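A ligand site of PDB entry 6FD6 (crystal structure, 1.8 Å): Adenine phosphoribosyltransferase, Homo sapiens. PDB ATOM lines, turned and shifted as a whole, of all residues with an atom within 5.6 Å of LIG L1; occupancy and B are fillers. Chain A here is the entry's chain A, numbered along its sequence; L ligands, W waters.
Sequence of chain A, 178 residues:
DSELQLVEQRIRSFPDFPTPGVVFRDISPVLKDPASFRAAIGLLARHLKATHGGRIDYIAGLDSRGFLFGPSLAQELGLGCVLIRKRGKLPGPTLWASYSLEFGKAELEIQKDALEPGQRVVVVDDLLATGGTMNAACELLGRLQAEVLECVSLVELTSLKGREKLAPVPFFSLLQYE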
ATOM      1  N   VAL A  23       9.899  -9.079 -24.054  1.00  0.00           N
ATOM      2  CA  VAL A  23      11.133  -8.799 -23.375  1.00  0.00           C
ATOM      3  C   VAL A  23      10.897  -9.011 -21.894  1.00  0.00           C
ATOM      4  O   VAL A  23      10.063  -8.349 -21.296  1.00  0.00           O
ATOM      5  CB  VAL A  23      11.605  -7.349 -23.681  1.00  0.00           C
ATOM      6  CG1 VAL A  23      12.863  -7.013 -22.902  1.00  0.00           C
ATOM      7  CG2 VAL A  23      11.843  -7.190 -25.166  1.00  0.00           C
ATOM      8  N   PHE A  24      11.604  -9.995 -21.326  1.00  0.00           N
ATOM      9  CA  PHE A  24      11.448 -10.355 -19.919  1.00  0.00           C
ATOM     10  C   PHE A  24      12.313  -9.463 -19.060  1.00  0.00           C
ATOM     11  O   PHE A  24      13.502  -9.319 -19.319  1.00  0.00           O
ATOM     12  CB  PHE A  24      11.823 -11.819 -19.706  1.00  0.00           C
ATOM     13  CG  PHE A  24      11.476 -12.332 -18.339  1.00  0.00           C
ATOM     14  CD1 PHE A  24      12.328 -12.149 -17.285  1.00  0.00           C
ATOM     15  CD2 PHE A  24      10.278 -12.998 -18.122  1.00  0.00           C
ATOM     16  CE1 PHE A  24      12.004 -12.611 -16.024  1.00  0.00           C
ATOM     17  CE2 PHE A  24       9.936 -13.473 -16.870  1.00  0.00           C
ATOM     18  CZ  PHE A  24      10.815 -13.282 -15.817  1.00  0.00           C
ATOM     19  N   ARG A  25      11.699  -8.829 -18.066  1.00  0.00           N
ATOM     20  CA  ARG A  25      12.411  -7.943 -17.163  1.00  0.00           C
ATOM     21  C   ARG A  25      12.711  -8.712 -15.907  1.00  0.00           C
ATOM     22  O   ARG A  25      11.802  -9.008 -15.124  1.00  0.00           O
ATOM     23  CB  ARG A  25      11.601  -6.686 -16.826  1.00  0.00           C
ATOM     24  CG  ARG A  25      11.047  -5.950 -18.023  1.00  0.00           C
ATOM     25  CD  ARG A  25      12.116  -5.431 -18.964  1.00  0.00           C
ATOM     26  NE  ARG A  25      11.449  -4.849 -20.138  1.00  0.00           N
ATOM     27  CZ  ARG A  25      12.032  -4.102 -21.057  1.00  0.00           C
ATOM     28  NH1 ARG A  25      13.323  -3.809 -20.975  1.00  0.00           N
ATOM     29  NH2 ARG A  25      11.321  -3.644 -22.071  1.00  0.00           N
ATOM     30  N   ASP A  26      13.983  -8.997 -15.710  1.00  0.00           N
ATOM     31  CA  ASP A  26      14.445  -9.859 -14.627  1.00  0.00           C
ATOM     32  C   ASP A  26      14.962  -9.042 -13.451  1.00  0.00           C
ATOM     33  O   ASP A  26      15.951  -8.315 -13.583  1.00  0.00           O
ATOM     34  CB  ASP A  26      15.566 -10.765 -15.161  1.00  0.00           C
ATOM     35  CG  ASP A  26      16.076 -11.758 -14.109  1.00  0.00           C
ATOM     36  OD1 ASP A  26      15.395 -11.968 -13.096  1.00  0.00           O
ATOM     37  OD2 ASP A  26      17.162 -12.342 -14.332  1.00  0.00           O
ATOM     38  N   ASP A  63       1.855 -13.815  -4.890  1.00  0.00           N
ATOM     39  CA  ASP A  63       2.579 -15.038  -5.262  1.00  0.00           C
ATOM     40  C   ASP A  63       2.972 -14.900  -6.749  1.00  0.00           C
ATOM     41  O   ASP A  63       2.114 -14.581  -7.554  1.00  0.00           O
ATOM     42  CB  ASP A  63       1.576 -16.183  -5.050  1.00  0.00           C
ATOM     43  CG  ASP A  63       2.192 -17.572  -5.038  1.00  0.00           C
ATOM     44  OD1 ASP A  63       3.434 -17.721  -5.198  1.00  0.00           O
ATOM     45  OD2 ASP A  63       1.400 -18.518  -4.857  1.00  0.00           O
ATOM     46  N   ARG A  65       6.609 -13.621  -7.164  1.00  0.00           N
ATOM     47  CA  ARG A  65       7.701 -12.649  -7.080  1.00  0.00           C
ATOM     48  C   ARG A  65       7.386 -11.486  -6.149  1.00  0.00           C
ATOM     49  O   ARG A  65       8.296 -10.835  -5.628  1.00  0.00           O
ATOM     50  CB  ARG A  65       8.112 -12.177  -8.465  1.00  0.00           C
ATOM     51  CG  ARG A  65       8.961 -13.209  -9.191  1.00  0.00           C
ATOM     52  CD  ARG A  65       9.265 -12.807 -10.622  1.00  0.00           C
ATOM     53  NE  ARG A  65       8.267 -13.374 -11.525  1.00  0.00           N
ATOM     54  CZ  ARG A  65       7.951 -12.875 -12.709  1.00  0.00           C
ATOM     55  NH1 ARG A  65       8.530 -11.760 -13.130  1.00  0.00           N
ATOM     56  NH2 ARG A  65       7.037 -13.477 -13.463  1.00  0.00           N
ATOM     57  N   TYR A  99      -8.702 -15.059 -13.661  1.00  0.00           N
ATOM     58  CA  TYR A  99      -8.243 -13.949 -14.460  1.00  0.00           C
ATOM     59  C   TYR A  99      -7.531 -14.591 -15.640  1.00  0.00           C
ATOM     60  O   TYR A  99      -7.239 -15.796 -15.602  1.00  0.00           O
ATOM     61  CB  TYR A  99      -7.331 -13.021 -13.627  1.00  0.00           C
ATOM     62  CG  TYR A  99      -6.027 -13.633 -13.180  1.00  0.00           C
ATOM     63  CD1 TYR A  99      -5.985 -14.533 -12.120  1.00  0.00           C
ATOM     64  CD2 TYR A  99      -4.839 -13.331 -13.831  1.00  0.00           C
ATOM     65  CE1 TYR A  99      -4.788 -15.115 -11.714  1.00  0.00           C
ATOM     66  CE2 TYR A  99      -3.639 -13.900 -13.428  1.00  0.00           C
ATOM     67  CZ  TYR A  99      -3.623 -14.790 -12.383  1.00  0.00           C
ATOM     68  OH  TYR A  99      -2.438 -15.363 -12.009  1.00  0.00           O
ATOM     69  N   SER A 100      -7.319 -13.817 -16.702  1.00  0.00           N
ATOM     70  CA  SER A 100      -6.662 -14.310 -17.903  1.00  0.00           C
ATOM     71  C   SER A 100      -5.149 -14.233 -17.706  1.00  0.00           C
ATOM     72  O   SER A 100      -4.640 -13.212 -17.230  1.00  0.00           O
ATOM     73  CB  SER A 100      -7.066 -13.465 -19.123  1.00  0.00           C
ATOM     74  OG  SER A 100      -6.856 -14.146 -20.350  1.00  0.00           O
ATOM     75  N   LEU A 101      -4.449 -15.305 -18.057  1.00  0.00           N
ATOM     76  CA  LEU A 101      -3.013 -15.331 -17.992  1.00  0.00           C
ATOM     77  C   LEU A 101      -2.484 -16.018 -19.249  1.00  0.00           C
ATOM     78  O   LEU A 101      -2.852 -17.156 -19.553  1.00  0.00           O
ATOM     79  CB  LEU A 101      -2.531 -16.067 -16.737  1.00  0.00           C
ATOM     80  CG  LEU A 101      -1.019 -16.196 -16.530  1.00  0.00           C
ATOM     81  CD1 LEU A 101      -0.371 -14.829 -16.310  1.00  0.00           C
ATOM     82  CD2 LEU A 101      -0.737 -17.132 -15.369  1.00  0.00           C
ATOM     83  N   ASP A 125       3.639  -6.167  -6.189  1.00  0.00           N
ATOM     84  CA  ASP A 125       4.159  -7.236  -7.035  1.00  0.00           C
ATOM     85  C   ASP A 125       5.428  -6.694  -7.666  1.00  0.00           C
ATOM     86  O   ASP A 125       5.737  -5.507  -7.524  1.00  0.00           O
ATOM     87  CB  ASP A 125       3.149  -7.626  -8.108  1.00  0.00           C
ATOM     88  CG  ASP A 125       3.337  -9.052  -8.620  1.00  0.00           C
ATOM     89  OD1 ASP A 125       4.307  -9.738  -8.208  1.00  0.00           O
ATOM     90  OD2 ASP A 125       2.471  -9.484  -9.427  1.00  0.00           O
ATOM     91  N   ASP A 126       6.210  -7.552  -8.318  1.00  0.00           N
ATOM     92  CA  ASP A 126       7.437  -7.081  -8.914  1.00  0.00           C
ATOM     93  C   ASP A 126       7.181  -6.237 -10.158  1.00  0.00           C
ATOM     94  O   ASP A 126       7.831  -5.225 -10.385  1.00  0.00           O
ATOM     95  CB  ASP A 126       8.405  -8.243  -9.204  1.00  0.00           C
ATOM     96  CG  ASP A 126       7.971  -9.147 -10.326  1.00  0.00           C
ATOM     97  OD1 ASP A 126       6.755  -9.414 -10.501  1.00  0.00           O
ATOM     98  OD2 ASP A 126       8.874  -9.648 -11.052  1.00  0.00           O
ATOM     99  N   LEU A 127       6.208  -6.659 -10.960  1.00  0.00           N
ATOM    100  CA  LEU A 127       5.987  -6.030 -12.256  1.00  0.00           C
ATOM    101  C   LEU A 127       4.521  -6.020 -12.605  1.00  0.00           C
ATOM    102  O   LEU A 127       3.806  -6.987 -12.344  1.00  0.00           O
ATOM    103  CB  LEU A 127       6.792  -6.787 -13.332  1.00  0.00           C
ATOM    104  CG  LEU A 127       6.666  -6.291 -14.783  1.00  0.00           C
ATOM    105  CD1 LEU A 127       7.963  -6.490 -15.524  1.00  0.00           C
ATOM    106  CD2 LEU A 127       5.525  -7.038 -15.485  1.00  0.00           C
ATOM    107  N   LEU A 128       4.085  -4.907 -13.184  1.00  0.00           N
ATOM    108  CA  LEU A 128       2.738  -4.740 -13.723  1.00  0.00           C
ATOM    109  C   LEU A 128       2.808  -4.806 -15.246  1.00  0.00           C
ATOM    110  O   LEU A 128       3.512  -4.021 -15.867  1.00  0.00           O
ATOM    111  CB  LEU A 128       2.148  -3.394 -13.305  1.00  0.00           C
ATOM    112  CG  LEU A 128       0.790  -3.064 -13.951  1.00  0.00           C
ATOM    113  CD1 LEU A 128      -0.268  -4.015 -13.455  1.00  0.00           C
ATOM    114  CD2 LEU A 128       0.351  -1.633 -13.717  1.00  0.00           C
ATOM    115  N   ALA A 129       2.076  -5.750 -15.826  1.00  0.00           N
ATOM    116  CA  ALA A 129       2.012  -5.877 -17.297  1.00  0.00           C
ATOM    117  C   ALA A 129       0.584  -5.580 -17.746  1.00  0.00           C
ATOM    118  O   ALA A 129       0.197  -4.438 -17.699  1.00  0.00           O
ATOM    119  CB  ALA A 129       2.487  -7.242 -17.749  1.00  0.00           C
ATOM    120  N   THR A 130      -0.223  -6.584 -18.122  1.00  0.00           N
ATOM    121  CA  THR A 130      -1.618  -6.303 -18.452  1.00  0.00           C
ATOM    122  C   THR A 130      -2.421  -5.794 -17.261  1.00  0.00           C
ATOM    123  O   THR A 130      -3.424  -5.103 -17.408  1.00  0.00           O
ATOM    124  CB  THR A 130      -2.381  -7.524 -19.035  1.00  0.00           C
ATOM    125  OG1 THR A 130      -2.603  -8.507 -18.016  1.00  0.00           O
ATOM    126  CG2 THR A 130      -1.613  -8.150 -20.187  1.00  0.00           C
ATOM    127  N   GLY A 131      -1.998  -6.134 -16.060  1.00  0.00           N
ATOM    128  CA  GLY A 131      -2.766  -5.764 -14.886  1.00  0.00           C
ATOM    129  C   GLY A 131      -3.736  -6.836 -14.440  1.00  0.00           C
ATOM    130  O   GLY A 131      -4.419  -6.662 -13.411  1.00  0.00           O
ATOM    131  N   GLY A 132      -3.838  -7.941 -15.185  1.00  0.00           N
ATOM    132  CA  GLY A 132      -4.805  -8.990 -14.823  1.00  0.00           C
ATOM    133  C   GLY A 132      -4.574  -9.540 -13.409  1.00  0.00           C
ATOM    134  O   GLY A 132      -5.526  -9.754 -12.666  1.00  0.00           O
ATOM    135  N   THR A 133      -3.312  -9.774 -13.070  1.00  0.00           N
ATOM    136  CA  THR A 133      -2.938 -10.321 -11.754  1.00  0.00           C
ATOM    137  C   THR A 133      -3.304  -9.348 -10.640  1.00  0.00           C
ATOM    138  O   THR A 133      -3.989  -9.718  -9.676  1.00  0.00           O
ATOM    139  CB  THR A 133      -1.431 -10.652 -11.740  1.00  0.00           C
ATOM    140  OG1 THR A 133      -1.143 -11.557 -12.802  1.00  0.00           O
ATOM    141  CG2 THR A 133      -0.955 -11.308 -10.411  1.00  0.00           C
ATOM    142  N   MET A 134      -2.862  -8.106 -10.758  1.00  0.00           N
ATOM    143  CA  MET A 134      -3.168  -7.106  -9.750  1.00  0.00           C
ATOM    144  C   MET A 134      -4.670  -6.844  -9.645  1.00  0.00           C
ATOM    145  O   MET A 134      -5.213  -6.633  -8.549  1.00  0.00           O
ATOM    146  CB  MET A 134      -2.443  -5.807 -10.106  1.00  0.00           C
ATOM    147  CG  MET A 134      -2.273  -4.858  -8.957  1.00  0.00           C
ATOM    148  SD  MET A 134      -1.075  -5.476  -7.774  1.00  0.00           S
ATOM    149  CE  MET A 134       0.475  -4.831  -8.397  1.00  0.00           C
ATOM    150  N   LEU A 157       5.062  -1.996 -17.491  1.00  0.00           N
ATOM    151  CA  LEU A 157       5.177  -2.055 -18.943  1.00  0.00           C
ATOM    152  C   LEU A 157       4.043  -1.224 -19.528  1.00  0.00           C
ATOM    153  O   LEU A 157       2.907  -1.690 -19.651  1.00  0.00           O
ATOM    154  CB  LEU A 157       5.155  -3.514 -19.418  1.00  0.00           C
ATOM    155  CG  LEU A 157       6.132  -4.465 -18.706  1.00  0.00           C
ATOM    156  CD1 LEU A 157       6.012  -5.881 -19.249  1.00  0.00           C
ATOM    157  CD2 LEU A 157       7.583  -3.970 -18.783  1.00  0.00           C
HETATM  158  P1  LIG L   1      -0.074  -9.194 -15.664  1.00  0.00           P
HETATM  159  O1  LIG L   1      -0.151  -9.312 -17.168  1.00  0.00           O
HETATM  160  O2  LIG L   1       0.117  -7.797 -15.162  1.00  0.00           O
HETATM  161  O3  LIG L   1      -1.138  -9.970 -14.915  1.00  0.00           O
HETATM  162  O4  LIG L   1       1.257 -10.037 -15.403  1.00  0.00           O
HETATM  163  C1  LIG L   1       1.998  -9.702 -14.254  1.00  0.00           C
HETATM  164  C2  LIG L   1       2.614 -10.961 -13.680  1.00  0.00           C
HETATM  165  O5  LIG L   1       3.356 -11.715 -14.645  1.00  0.00           O
HETATM  166  C3  LIG L   1       3.567 -10.422 -12.658  1.00  0.00           C
HETATM  167  O6  LIG L   1       3.468 -11.258 -11.499  1.00  0.00           O
HETATM  168  C4  LIG L   1       4.892 -10.425 -13.394  1.00  0.00           C
HETATM  169  O7  LIG L   1       5.896 -10.891 -12.505  1.00  0.00           O
HETATM  170  C5  LIG L   1       4.747 -11.346 -14.621  1.00  0.00           C
HETATM  171  N1  LIG L   1       5.201 -10.712 -15.908  1.00  0.00           N
HETATM  172  C6  LIG L   1       4.401 -10.301 -16.925  1.00  0.00           C
HETATM  173  N2  LIG L   1       5.118  -9.760 -17.954  1.00  0.00           N
HETATM  174  C7  LIG L   1       6.439  -9.825 -17.602  1.00  0.00           C
HETATM  175  C8  LIG L   1       7.742  -9.431 -18.200  1.00  0.00           C
HETATM  176  N3  LIG L   1       7.806  -8.849 -19.422  1.00  0.00           N
HETATM  177  N4  LIG L   1       8.877  -9.660 -17.498  1.00  0.00           N
HETATM  178  C9  LIG L   1       8.842 -10.243 -16.281  1.00  0.00           C
HETATM  179  N5  LIG L   1       7.700 -10.626 -15.675  1.00  0.00           N
HETATM  180  C10 LIG L   1       6.476 -10.451 -16.253  1.00  0.00           C
HETATM  181  O1  LG2 L   2       2.249 -15.440 -12.920  1.00  0.00           O
HETATM  182  P1  LG2 L   2       3.690 -14.982 -12.969  1.00  0.00           P
HETATM  183  O2  LG2 L   2       3.899 -13.600 -12.362  1.00  0.00           O
HETATM  184  O3  LG2 L   2       4.307 -15.186 -14.333  1.00  0.00           O
HETATM  185  O4  LG2 L   2       4.449 -16.080 -12.056  1.00  0.00           O
HETATM  186  P2  LG2 L   2       5.566 -15.922 -10.886  1.00  0.00           P
HETATM  187  O5  LG2 L   2       5.138 -14.802  -9.960  1.00  0.00           O
HETATM  188  O6  LG2 L   2       5.502 -17.330 -10.302  1.00  0.00           O
HETATM  189  O7  LG2 L   2       6.850 -15.651 -11.608  1.00  0.00           O
HETATM  190  O   HOH W   1       1.201 -10.699 -18.883  1.00  0.00           O
HETATM  191  O   HOH W   2       3.685  -9.527 -20.263  1.00  0.00           O
HETATM  192  O   HOH W   3      -0.848  -7.441 -12.580  1.00  0.00           O
HETATM  193  O   HOH W   4       6.237 -13.728 -16.434  1.00  0.00           O
HETATM  194  O   HOH W   5      -2.825 -11.512 -16.483  1.00  0.00           O
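Water W5 lies within hydrogen-bond range of O of Ser 100 (2.6 Å), O3 of LIG L1 (2.8 Å) and OG1 of Thr 130 (3.4 Å). Water W3 lies within hydrogen-bond range of an oxygen (O2) of LIG L1 (2.8 Å), the backbone NH (N) of Met 134 (2.8 Å) and the backbone NH (N) of Thr 133 (3.4 Å). Water W4 lies within hydrogen-bond range of the guanidinium group of Arg 65 and an oxygen (O3) of LG2 L2.
O7 of LIG L1 is in hydrogen-bond range of OD1 of Asp 126, 2.6 Å away. An oxygen (O1) of LIG L1 sits at hydrogen-bond distance from the backbone NH (N) of Thr 130 (2.9 Å). OG1 of Thr 130 is in hydrogen-bond range of O1 of LIG L1. O5 of LG2 L2 is in hydrogen-bond range of N of Arg 65 (3.4 Å). The backbone carbonyl oxygen of Val 23 is in hydrogen-bond range of a nitrogen (N3) of LIG L1 (3.0 Å). N of Arg 25 sits at hydrogen-bond distance from N4 of LIG L1, 3.0 Å away. O7 of LIG L1 lies within hydrogen-bond range of NH1 of Arg 65. OG1 of Thr 133 sits at hydrogen-bond distance from O3 of LIG L1 (2.6 Å). OD2 of Asp 125 is in hydrogen-bond range of O6 of LIG L1 (2.9 Å). The backbone NH (N) of Gly 131 lies within hydrogen-bond range of an oxygen (O2) of LIG L1 (2.8 Å). The backbone NH (N) of Gly 132 is in hydrogen-bond range of an oxygen (O3) of LIG L1, at 3.4 Å. NE of Arg 65 lies within salt-bridge range of O7 of LG2 L2, 2.7 Å away. An oxygen (O3) of LIG L1 sits at hydrogen-bond distance from the backbone NH (N) of Thr 133 (2.9 Å). O2 of LIG L1 lies within hydrogen-bond range of N of Ala 129 (2.9 Å).
The backbone carbonyl oxygen of Leu 128 is in hydrogen-bond range of the backbone NH of Leu 157 (3.0 Å). The side-chain carboxylate (OD2) of Asp 126 is in salt-bridge range of the guanidinium group (NH1) of Arg 65 (3.0 Å). The backbone NH (N) of Gly 132 is in hydrogen-bond range of the side-chain hydroxyl (OG1) of Thr 130, 3.1 Å away.
Phe 24 touches LIG L1. Leu 127 touches LIG L1. Leu 157 touches LIG L1 (CD1 to N3, 3.5 Å). Hydrophobic or aromatic side chains that line LIG L1: Phe 24, Leu 127, Ala 129 and Leu 157. The nearest printed residue that does not touch LIG L1 is Leu 128 (4.02 Å).
O6 of LIG L1 is in hydrogen-bond range of O2 of LG2 L2, 2.5 Å away.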
